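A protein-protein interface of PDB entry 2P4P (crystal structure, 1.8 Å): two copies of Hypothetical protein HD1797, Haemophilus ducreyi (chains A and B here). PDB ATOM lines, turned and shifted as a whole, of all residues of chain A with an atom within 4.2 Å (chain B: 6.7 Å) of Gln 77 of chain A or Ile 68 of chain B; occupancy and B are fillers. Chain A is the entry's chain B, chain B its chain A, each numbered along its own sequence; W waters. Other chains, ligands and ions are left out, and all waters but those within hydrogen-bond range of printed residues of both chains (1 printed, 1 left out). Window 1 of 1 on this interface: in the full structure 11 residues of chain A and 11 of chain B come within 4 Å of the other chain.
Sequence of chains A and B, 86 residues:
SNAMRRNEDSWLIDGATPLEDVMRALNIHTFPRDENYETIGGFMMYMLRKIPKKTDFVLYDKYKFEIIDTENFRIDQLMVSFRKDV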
ATOM      1  N   ILE A  13     -23.544  27.878  27.317  1.00  0.00           N
ATOM      2  CA  ILE A  13     -24.904  28.308  27.729  1.00  0.00           C
ATOM      3  C   ILE A  13     -25.341  29.481  26.846  1.00  0.00           C
ATOM      4  O   ILE A  13     -24.511  30.301  26.421  1.00  0.00           O
ATOM      5  CB  ILE A  13     -24.907  28.745  29.238  1.00  0.00           C
ATOM      6  CG1 ILE A  13     -24.639  27.518  30.130  1.00  0.00           C
ATOM      7  CG2 ILE A  13     -26.255  29.398  29.664  1.00  0.00           C
ATOM      8  CD1 ILE A  13     -24.283  27.841  31.600  1.00  0.00           C
ATOM      9  N   ASP A  14     -26.634  29.563  26.574  1.00  0.00           N
ATOM     10  CA  ASP A  14     -27.182  30.684  25.803  1.00  0.00           C
ATOM     11  C   ASP A  14     -27.319  31.919  26.688  1.00  0.00           C
ATOM     12  O   ASP A  14     -27.771  31.829  27.846  1.00  0.00           O
ATOM     13  CB  ASP A  14     -28.557  30.328  25.264  1.00  0.00           C
ATOM     14  CG  ASP A  14     -28.500  29.354  24.140  1.00  0.00           C
ATOM     15  OD1 ASP A  14     -27.421  28.779  23.872  1.00  0.00           O
ATOM     16  OD2 ASP A  14     -29.559  29.148  23.526  1.00  0.00           O
ATOM     17  N   ILE A  67     -17.565  35.413  27.281  1.00  0.00           N
ATOM     18  CA  ILE A  67     -18.335  35.667  26.073  1.00  0.00           C
ATOM     19  C   ILE A  67     -17.762  34.887  24.912  1.00  0.00           C
ATOM     20  O   ILE A  67     -16.603  35.100  24.521  1.00  0.00           O
ATOM     21  CB  ILE A  67     -18.397  37.172  25.731  1.00  0.00           C
ATOM     22  CG1 ILE A  67     -18.966  37.979  26.923  1.00  0.00           C
ATOM     23  CG2 ILE A  67     -19.267  37.387  24.487  1.00  0.00           C
ATOM     24  CD1 ILE A  67     -18.984  39.523  26.706  1.00  0.00           C
ATOM     25  N   ILE A  68     -18.581  33.985  24.368  1.00  0.00           N
ATOM     26  CA  ILE A  68     -18.218  33.217  23.153  1.00  0.00           C
ATOM     27  C   ILE A  68     -18.747  33.888  21.889  1.00  0.00           C
ATOM     28  O   ILE A  68     -18.061  33.919  20.879  1.00  0.00           O
ATOM     29  CB  ILE A  68     -18.721  31.739  23.241  1.00  0.00           C
ATOM     30  CG1 ILE A  68     -18.055  31.017  24.430  1.00  0.00           C
ATOM     31  CG2 ILE A  68     -18.505  30.956  21.895  1.00  0.00           C
ATOM     32  CD1 ILE A  68     -16.470  30.907  24.391  1.00  0.00           C
ATOM     33  N   ASP A  69     -19.964  34.427  21.947  1.00  0.00           N
ATOM     34  CA  ASP A  69     -20.478  35.194  20.822  1.00  0.00           C
ATOM     35  C   ASP A  69     -21.406  36.284  21.272  1.00  0.00           C
ATOM     36  O   ASP A  69     -22.175  36.090  22.236  1.00  0.00           O
ATOM     37  CB  ASP A  69     -21.204  34.271  19.821  1.00  0.00           C
ATOM     38  CG  ASP A  69     -21.664  35.015  18.560  1.00  0.00           C
ATOM     39  OD1 ASP A  69     -20.855  35.745  17.926  1.00  0.00           O
ATOM     40  OD2 ASP A  69     -22.844  34.854  18.184  1.00  0.00           O
ATOM     41  N   ILE A  75     -25.220  39.372  24.582  1.00  0.00           N
ATOM     42  CA  ILE A  75     -24.296  38.230  24.711  1.00  0.00           C
ATOM     43  C   ILE A  75     -25.097  37.012  24.296  1.00  0.00           C
ATOM     44  O   ILE A  75     -26.144  36.719  24.906  1.00  0.00           O
ATOM     45  CB  ILE A  75     -23.789  38.039  26.149  1.00  0.00           C
ATOM     46  CG1 ILE A  75     -22.947  39.248  26.573  1.00  0.00           C
ATOM     47  CG2 ILE A  75     -23.024  36.656  26.286  1.00  0.00           C
ATOM     48  CD1 ILE A  75     -22.645  39.300  28.087  1.00  0.00           C
ATOM     49  N   ASP A  76     -24.652  36.335  23.229  1.00  0.00           N
ATOM     50  CA  ASP A  76     -25.500  35.308  22.644  1.00  0.00           C
ATOM     51  C   ASP A  76     -25.176  33.938  23.236  1.00  0.00           C
ATOM     52  O   ASP A  76     -26.088  33.195  23.608  1.00  0.00           O
ATOM     53  CB  ASP A  76     -25.367  35.265  21.127  1.00  0.00           C
ATOM     54  CG  ASP A  76     -26.419  34.373  20.484  1.00  0.00           C
ATOM     55  OD1 ASP A  76     -27.637  34.606  20.692  1.00  0.00           O
ATOM     56  OD2 ASP A  76     -26.024  33.435  19.794  1.00  0.00           O
ATOM     57  N   GLN A  77     -23.883  33.629  23.282  1.00  0.00           N
ATOM     58  CA  GLN A  77     -23.368  32.389  23.878  1.00  0.00           C
ATOM     59  C   GLN A  77     -22.248  32.682  24.872  1.00  0.00           C
ATOM     60  O   GLN A  77     -21.371  33.540  24.633  1.00  0.00           O
ATOM     61  CB  GLN A  77     -22.811  31.439  22.806  1.00  0.00           C
ATOM     62  CG  GLN A  77     -23.760  31.094  21.643  1.00  0.00           C
ATOM     63  CD  GLN A  77     -24.725  29.960  21.945  1.00  0.00           C
ATOM     64  OE1 GLN A  77     -24.695  29.350  23.019  1.00  0.00           O
ATOM     65  NE2 GLN A  77     -25.598  29.670  20.977  1.00  0.00           N
ATOM     66  N   LEU A  78     -22.202  31.904  25.937  1.00  0.00           N
ATOM     67  CA  LEU A  78     -21.154  32.066  26.913  1.00  0.00           C
ATOM     68  C   LEU A  78     -20.631  30.700  27.323  1.00  0.00           C
ATOM     69  O   LEU A  78     -21.304  29.697  27.114  1.00  0.00           O
ATOM     70  CB  LEU A  78     -21.654  32.813  28.141  1.00  0.00           C
ATOM     71  CG  LEU A  78     -22.765  32.132  28.967  1.00  0.00           C
ATOM     72  CD1 LEU A  78     -22.375  32.022  30.439  1.00  0.00           C
ATOM     73  CD2 LEU A  78     -24.070  32.847  28.789  1.00  0.00           C
ATOM     74  N   ARG B   5     -28.543  23.063  27.779  1.00  0.00           N
ATOM     75  CA  ARG B   5     -28.010  21.748  27.488  1.00  0.00           C
ATOM     76  C   ARG B   5     -27.411  21.155  28.744  1.00  0.00           C
ATOM     77  O   ARG B   5     -26.887  21.885  29.591  1.00  0.00           O
ATOM     78  CB  ARG B   5     -26.930  21.827  26.410  1.00  0.00           C
ATOM     79  CG  ARG B   5     -25.605  22.408  26.885  1.00  0.00           C
ATOM     80  CD  ARG B   5     -24.512  22.309  25.835  1.00  0.00           C
ATOM     81  NE  ARG B   5     -24.587  23.423  24.894  1.00  0.00           N
ATOM     82  CZ  ARG B   5     -25.133  23.350  23.687  1.00  0.00           C
ATOM     83  NH1 ARG B   5     -25.629  22.200  23.252  1.00  0.00           N
ATOM     84  NH2 ARG B   5     -25.157  24.422  22.910  1.00  0.00           N
ATOM     85  N   LEU B  12     -14.996  23.194  21.885  1.00  0.00           N
ATOM     86  CA  LEU B  12     -15.355  24.321  21.050  1.00  0.00           C
ATOM     87  C   LEU B  12     -14.269  24.509  20.013  1.00  0.00           C
ATOM     88  O   LEU B  12     -13.088  24.688  20.356  1.00  0.00           O
ATOM     89  CB  LEU B  12     -15.521  25.571  21.905  1.00  0.00           C
ATOM     90  CG  LEU B  12     -16.023  26.826  21.195  1.00  0.00           C
ATOM     91  CD1 LEU B  12     -17.522  26.728  20.943  1.00  0.00           C
ATOM     92  CD2 LEU B  12     -15.716  28.036  22.046  1.00  0.00           C
ATOM     93  N   MET B  44     -19.643  20.602   7.433  1.00  0.00           N
ATOM     94  CA  MET B  44     -20.917  20.697   8.162  1.00  0.00           C
ATOM     95  C   MET B  44     -22.001  21.347   7.313  1.00  0.00           C
ATOM     96  O   MET B  44     -23.137  20.869   7.279  1.00  0.00           O
ATOM     97  CB  MET B  44     -20.741  21.486   9.472  1.00  0.00           C
ATOM     98  CG  MET B  44     -20.009  20.716  10.547  1.00  0.00           C
ATOM     99  SD  MET B  44     -19.915  21.888  12.121  1.00  0.00           S
ATOM    100  CE  MET B  44     -21.773  21.858  12.662  1.00  0.00           C
ATOM    101  N   MLY B  53     -27.550  27.888  10.603  1.00  0.00           N
ATOM    102  CA  MLY B  53     -27.841  28.831  11.683  1.00  0.00           C
ATOM    103  CB  MLY B  53     -29.285  29.292  11.660  1.00  0.00           C
ATOM    104  CG  MLY B  53     -30.304  28.174  11.566  1.00  0.00           C
ATOM    105  CD  MLY B  53     -31.712  28.778  11.608  1.00  0.00           C
ATOM    106  CE  MLY B  53     -32.752  27.844  12.220  1.00  0.00           C
ATOM    107  NZ  MLY B  53     -32.416  26.422  12.013  1.00  0.00           N
ATOM    108  CH1 MLY B  53     -32.867  25.626  13.168  1.00  0.00           C
ATOM    109  CH2 MLY B  53     -33.060  25.871  10.801  1.00  0.00           C
ATOM    110  C   MLY B  53     -27.486  28.215  13.000  1.00  0.00           C
ATOM    111  O   MLY B  53     -27.422  26.993  13.101  1.00  0.00           O
ATOM    112  N   MLY B  54     -27.276  29.050  14.021  1.00  0.00           N
ATOM    113  CA  MLY B  54     -26.925  28.590  15.367  1.00  0.00           C
ATOM    114  CB  MLY B  54     -26.777  29.772  16.351  1.00  0.00           C
ATOM    115  CG  MLY B  54     -28.102  30.463  16.614  1.00  0.00           C
ATOM    116  CD  MLY B  54     -28.014  31.665  17.555  1.00  0.00           C
ATOM    117  CE  MLY B  54     -29.308  31.679  18.367  1.00  0.00           C
ATOM    118  NZ  MLY B  54     -29.285  32.710  19.413  1.00  0.00           N
ATOM    119  CH1 MLY B  54     -30.427  33.615  19.230  1.00  0.00           C
ATOM    120  CH2 MLY B  54     -29.304  32.047  20.729  1.00  0.00           C
ATOM    121  C   MLY B  54     -27.936  27.578  15.839  1.00  0.00           C
ATOM    122  O   MLY B  54     -29.135  27.731  15.573  1.00  0.00           O
ATOM    123  N   THR B  55     -27.438  26.556  16.539  1.00  0.00           N
ATOM    124  CA  THR B  55     -28.185  25.393  17.031  1.00  0.00           C
ATOM    125  C   THR B  55     -28.332  24.246  16.016  1.00  0.00           C
ATOM    126  O   THR B  55     -28.553  23.100  16.411  1.00  0.00           O
ATOM    127  CB  THR B  55     -29.582  25.730  17.676  1.00  0.00           C
ATOM    128  OG1 THR B  55     -30.555  25.953  16.652  1.00  0.00           O
ATOM    129  CG2 THR B  55     -29.499  26.934  18.595  1.00  0.00           C
ATOM    130  N   ASP B  56     -28.190  24.528  14.719  1.00  0.00           N
ATOM    131  CA  ASP B  56     -28.230  23.432  13.744  1.00  0.00           C
ATOM    132  C   ASP B  56     -27.090  22.483  14.097  1.00  0.00           C
ATOM    133  O   ASP B  56     -26.046  22.918  14.600  1.00  0.00           O
ATOM    134  CB  ASP B  56     -28.001  23.906  12.303  1.00  0.00           C
ATOM    135  CG  ASP B  56     -29.156  24.708  11.736  1.00  0.00           C
ATOM    136  OD1 ASP B  56     -30.234  24.793  12.367  1.00  0.00           O
ATOM    137  OD2 ASP B  56     -28.978  25.265  10.636  1.00  0.00           O
ATOM    138  N   GLU B  66     -22.453  20.847  16.552  1.00  0.00           N
ATOM    139  CA  GLU B  66     -23.481  21.888  16.687  1.00  0.00           C
ATOM    140  C   GLU B  66     -22.920  23.264  16.320  1.00  0.00           C
ATOM    141  O   GLU B  66     -21.901  23.688  16.880  1.00  0.00           O
ATOM    142  CB  GLU B  66     -24.032  21.925  18.111  1.00  0.00           C
ATOM    143  CG  GLU B  66     -25.193  22.903  18.314  1.00  0.00           C
ATOM    144  CD  GLU B  66     -25.827  22.841  19.699  1.00  0.00           C
ATOM    145  OE1 GLU B  66     -25.829  21.759  20.331  1.00  0.00           O
ATOM    146  OE2 GLU B  66     -26.339  23.892  20.153  1.00  0.00           O
ATOM    147  N   ILE B  67     -23.575  23.975  15.405  1.00  0.00           N
ATOM    148  CA  ILE B  67     -23.170  25.377  15.110  1.00  0.00           C
ATOM    149  C   ILE B  67     -23.384  26.310  16.317  1.00  0.00           C
ATOM    150  O   ILE B  67     -24.498  26.434  16.841  1.00  0.00           O
ATOM    151  CB  ILE B  67     -23.907  25.975  13.876  1.00  0.00           C
ATOM    152  CG1 ILE B  67     -23.609  25.189  12.601  1.00  0.00           C
ATOM    153  CG2 ILE B  67     -23.579  27.496  13.734  1.00  0.00           C
ATOM    154  CD1 ILE B  67     -24.486  25.668  11.395  1.00  0.00           C
ATOM    155  N   ILE B  68     -22.315  26.957  16.779  1.00  0.00           N
ATOM    156  CA  ILE B  68     -22.467  27.907  17.874  1.00  0.00           C
ATOM    157  C   ILE B  68     -22.796  29.288  17.311  1.00  0.00           C
ATOM    158  O   ILE B  68     -23.696  29.986  17.796  1.00  0.00           O
ATOM    159  CB  ILE B  68     -21.234  27.898  18.845  1.00  0.00           C
ATOM    160  CG1 ILE B  68     -21.182  26.548  19.587  1.00  0.00           C
ATOM    161  CG2 ILE B  68     -21.234  29.132  19.820  1.00  0.00           C
ATOM    162  CD1 ILE B  68     -22.556  26.094  20.205  1.00  0.00           C
ATOM    163  N   ASP B  69     -22.072  29.664  16.271  1.00  0.00           N
ATOM    164  CA  ASP B  69     -22.389  30.881  15.542  1.00  0.00           C
ATOM    165  C   ASP B  69     -21.877  30.875  14.092  1.00  0.00           C
ATOM    166  O   ASP B  69     -20.901  30.194  13.757  1.00  0.00           O
ATOM    167  CB  ASP B  69     -21.892  32.099  16.324  1.00  0.00           C
ATOM    168  CG  ASP B  69     -20.392  32.302  16.216  1.00  0.00           C
ATOM    169  OD1 ASP B  69     -19.996  33.284  15.566  1.00  0.00           O
ATOM    170  OD2 ASP B  69     -19.604  31.505  16.772  1.00  0.00           O
ATOM    171  N   THR B  70     -22.566  31.629  13.244  1.00  0.00           N
ATOM    172  CA  THR B  70     -22.099  31.897  11.903  1.00  0.00           C
ATOM    173  C   THR B  70     -21.617  33.359  11.841  1.00  0.00           C
ATOM    174  O   THR B  70     -22.056  34.213  12.624  1.00  0.00           O
ATOM    175  CB  THR B  70     -23.183  31.642  10.812  1.00  0.00           C
ATOM    176  OG1 THR B  70     -24.242  32.599  10.942  1.00  0.00           O
ATOM    177  CG2 THR B  70     -23.755  30.200  10.900  1.00  0.00           C
ATOM    178  N   ILE B  75     -19.642  28.976   9.070  1.00  0.00           N
ATOM    179  CA  ILE B  75     -19.680  28.495  10.438  1.00  0.00           C
ATOM    180  C   ILE B  75     -18.403  29.010  11.080  1.00  0.00           C
ATOM    181  O   ILE B  75     -17.287  28.705  10.631  1.00  0.00           O
ATOM    182  CB  ILE B  75     -19.810  26.940  10.512  1.00  0.00           C
ATOM    183  CG1 ILE B  75     -21.143  26.510   9.872  1.00  0.00           C
ATOM    184  CG2 ILE B  75     -19.646  26.455  11.948  1.00  0.00           C
ATOM    185  CD1 ILE B  75     -21.374  25.001   9.706  1.00  0.00           C
ATOM    186  N   ASP B  76     -18.573  29.866  12.078  1.00  0.00           N
ATOM    187  CA  ASP B  76     -17.468  30.539  12.761  1.00  0.00           C
ATOM    188  C   ASP B  76     -16.960  29.639  13.916  1.00  0.00           C
ATOM    189  O   ASP B  76     -15.749  29.335  14.008  1.00  0.00           O
ATOM    190  CB  ASP B  76     -17.986  31.907  13.242  1.00  0.00           C
ATOM    191  CG  ASP B  76     -17.012  32.658  14.110  1.00  0.00           C
ATOM    192  OD1 ASP B  76     -15.799  32.688  13.811  1.00  0.00           O
ATOM    193  OD2 ASP B  76     -17.478  33.269  15.091  1.00  0.00           O
ATOM    194  N   GLN B  77     -17.888  29.222  14.774  1.00  0.00           N
ATOM    195  CA  GLN B  77     -17.590  28.284  15.874  1.00  0.00           C
ATOM    196  C   GLN B  77     -18.592  27.159  15.963  1.00  0.00           C
ATOM    197  O   GLN B  77     -19.781  27.369  15.759  1.00  0.00           O
ATOM    198  CB  GLN B  77     -17.584  28.998  17.214  1.00  0.00           C
ATOM    199  CG  GLN B  77     -16.435  29.937  17.385  1.00  0.00           C
ATOM    200  CD  GLN B  77     -16.493  30.655  18.705  1.00  0.00           C
ATOM    201  OE1 GLN B  77     -15.606  30.519  19.525  1.00  0.00           O
ATOM    202  NE2 GLN B  77     -17.547  31.407  18.920  1.00  0.00           N
ATOM    203  N   LEU B  78     -18.107  25.973  16.325  1.00  0.00           N
ATOM    204  CA  LEU B  78     -18.951  24.827  16.553  1.00  0.00           C
ATOM    205  C   LEU B  78     -18.544  24.110  17.846  1.00  0.00           C
ATOM    206  O   LEU B  78     -17.448  24.303  18.362  1.00  0.00           O
ATOM    207  CB  LEU B  78     -18.841  23.847  15.386  1.00  0.00           C
ATOM    208  CG  LEU B  78     -17.409  23.384  15.092  1.00  0.00           C
ATOM    209  CD1 LEU B  78     -17.292  21.856  15.139  1.00  0.00           C
ATOM    210  CD2 LEU B  78     -16.894  23.980  13.771  1.00  0.00           C
ATOM    211  N   MET B  79     -19.444  23.293  18.361  1.00  0.00           N
ATOM    212  CA  MET B  79     -19.151  22.441  19.487  1.00  0.00           C
ATOM    213  C   MET B  79     -19.307  21.002  19.065  1.00  0.00           C
ATOM    214  O   MET B  79     -20.209  20.673  18.301  1.00  0.00           O
ATOM    215  CB  MET B  79     -20.151  22.704  20.609  1.00  0.00           C
ATOM    216  CG  MET B  79     -19.712  22.137  21.940  1.00  0.00           C
ATOM    217  SD  MET B  79     -21.162  22.347  23.209  1.00  0.00           S
ATOM    218  CE  MET B  79     -22.571  22.758  21.974  1.00  0.00           C
HETATM  219  O   HOH W   1     -26.054  26.639  19.876  1.00  0.00           O
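NZ of MLY 54 of chain B lies close to OD1 of Asp 76 of chain A (2.8 Å).
The side-chain amide nitrogen (NE2) of Gln 77 of chain B sits close to the backbone carbonyl oxygen (O) of Ile 68 of chain A, 3.2 Å away.
O of Asp 69 of chain B is in hydrogen-bond range of N of Asp 76 of chain B (2.9 Å).
The side-chain amide nitrogen (NE2) of Gln 77 of chain B is in hydrogen-bond range of the side-chain carboxylate (OD2) of Asp 69 of chain B, at 3.0 Å.
The side-chain carboxylate of Asp 14 of chain A lies close to the side-chain amide oxygen of Gln 77 of chain A (2.9 Å).
The backbone NH of Ile 68 of chain A lies within hydrogen-bond range of the backbone carbonyl oxygen of Gln 77 of chain A, 2.8 Å away.
N of Asp 76 of chain A lies within hydrogen-bond range of O of Asp 69 of chain A (2.7 Å).
N of Asp 69 of chain A sits at hydrogen-bond distance from O of Gln 77 of chain A, at 3.2 Å.
Among the printed residues, pairs that only touch across the chains: Ile 68 of chain A with Leu 12 of chain B, Ile 68 of chain A with Ile 68 of chain B, Asp 69 of chain A with Asp 69 of chain B and Gln 77 of chain A with Ile 68 of chain B.
Of the printed residues of chain B, Ile 68 of chain A touches Leu 12 (3.8 Å), Ile 68 (3.9 Å) and Gln 77 (3.2 Å).
Printed residues of chain B within 4 Å of Asp 69 of chain A: Asp 69 (3.5 Å).
Ile 75 of chain A touches none of the printed residues of chain B.
Of the printed residues of chain B, Asp 76 of chain A touches MLY 54 (2.8 Å).
Gln 77 of chain A touches one residue of chain B.
Leu 78 of chain A touches none of the printed residues of chain B.
Printed residues of chain A within 4 Å of Leu 12 of chain B: Ile 68 (3.8 Å).
Ile 68 of chain B touches just these residues of chain A: Ile 68 (3.9 Å) and Gln 77 (3.7 Å).
The nearest printed residue of chain A that does not touch Leu 12 of chain B is Gln 77 of chain A (7.3 Å).
Hydrophobic or aromatic side chains of chain B that line the printed part of chain A: Leu 12 and Ile 68.
Of the 9 printed residues of chain A, 4 touch a printed residue of chain B.
Printed residues of chain A that touch a printed residue of chain B: Ile 68, Asp 69, Asp 76 and Gln 77.
Hydrophobic or aromatic side chains of chain A within 4 Å of the printed part of chain B: Ile 68.
Along chain A the printed residues that touch a printed residue of chain B span positions 68 to 77.
Among the printed residues, 6 pairs touch across the chains.
Among the printed residues, no Asp or Glu carboxylate lies within 4 Å of a Lys or Arg side-chain nitrogen of the other chain.
Ile 68 of chain B touches its own counterpart, Ile 68 of chain A.
Ile 68 of chain A touches Gln 77 of chain B, and with the chains exchanged Gln 77 of chain A touches Ile 68 of chain B.
Asp 69 of chain A touches its own counterpart, Asp 69 of chain B.
Of the 6 pairs that touch across the chains among the printed residues, 4 have their exchanged pair printed and touching as well.
Water W1 lies within hydrogen-bond range of OE2 of Glu 66 of chain B, NE2 of Gln 77 of chain A and O of Ile 67 of chain B.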
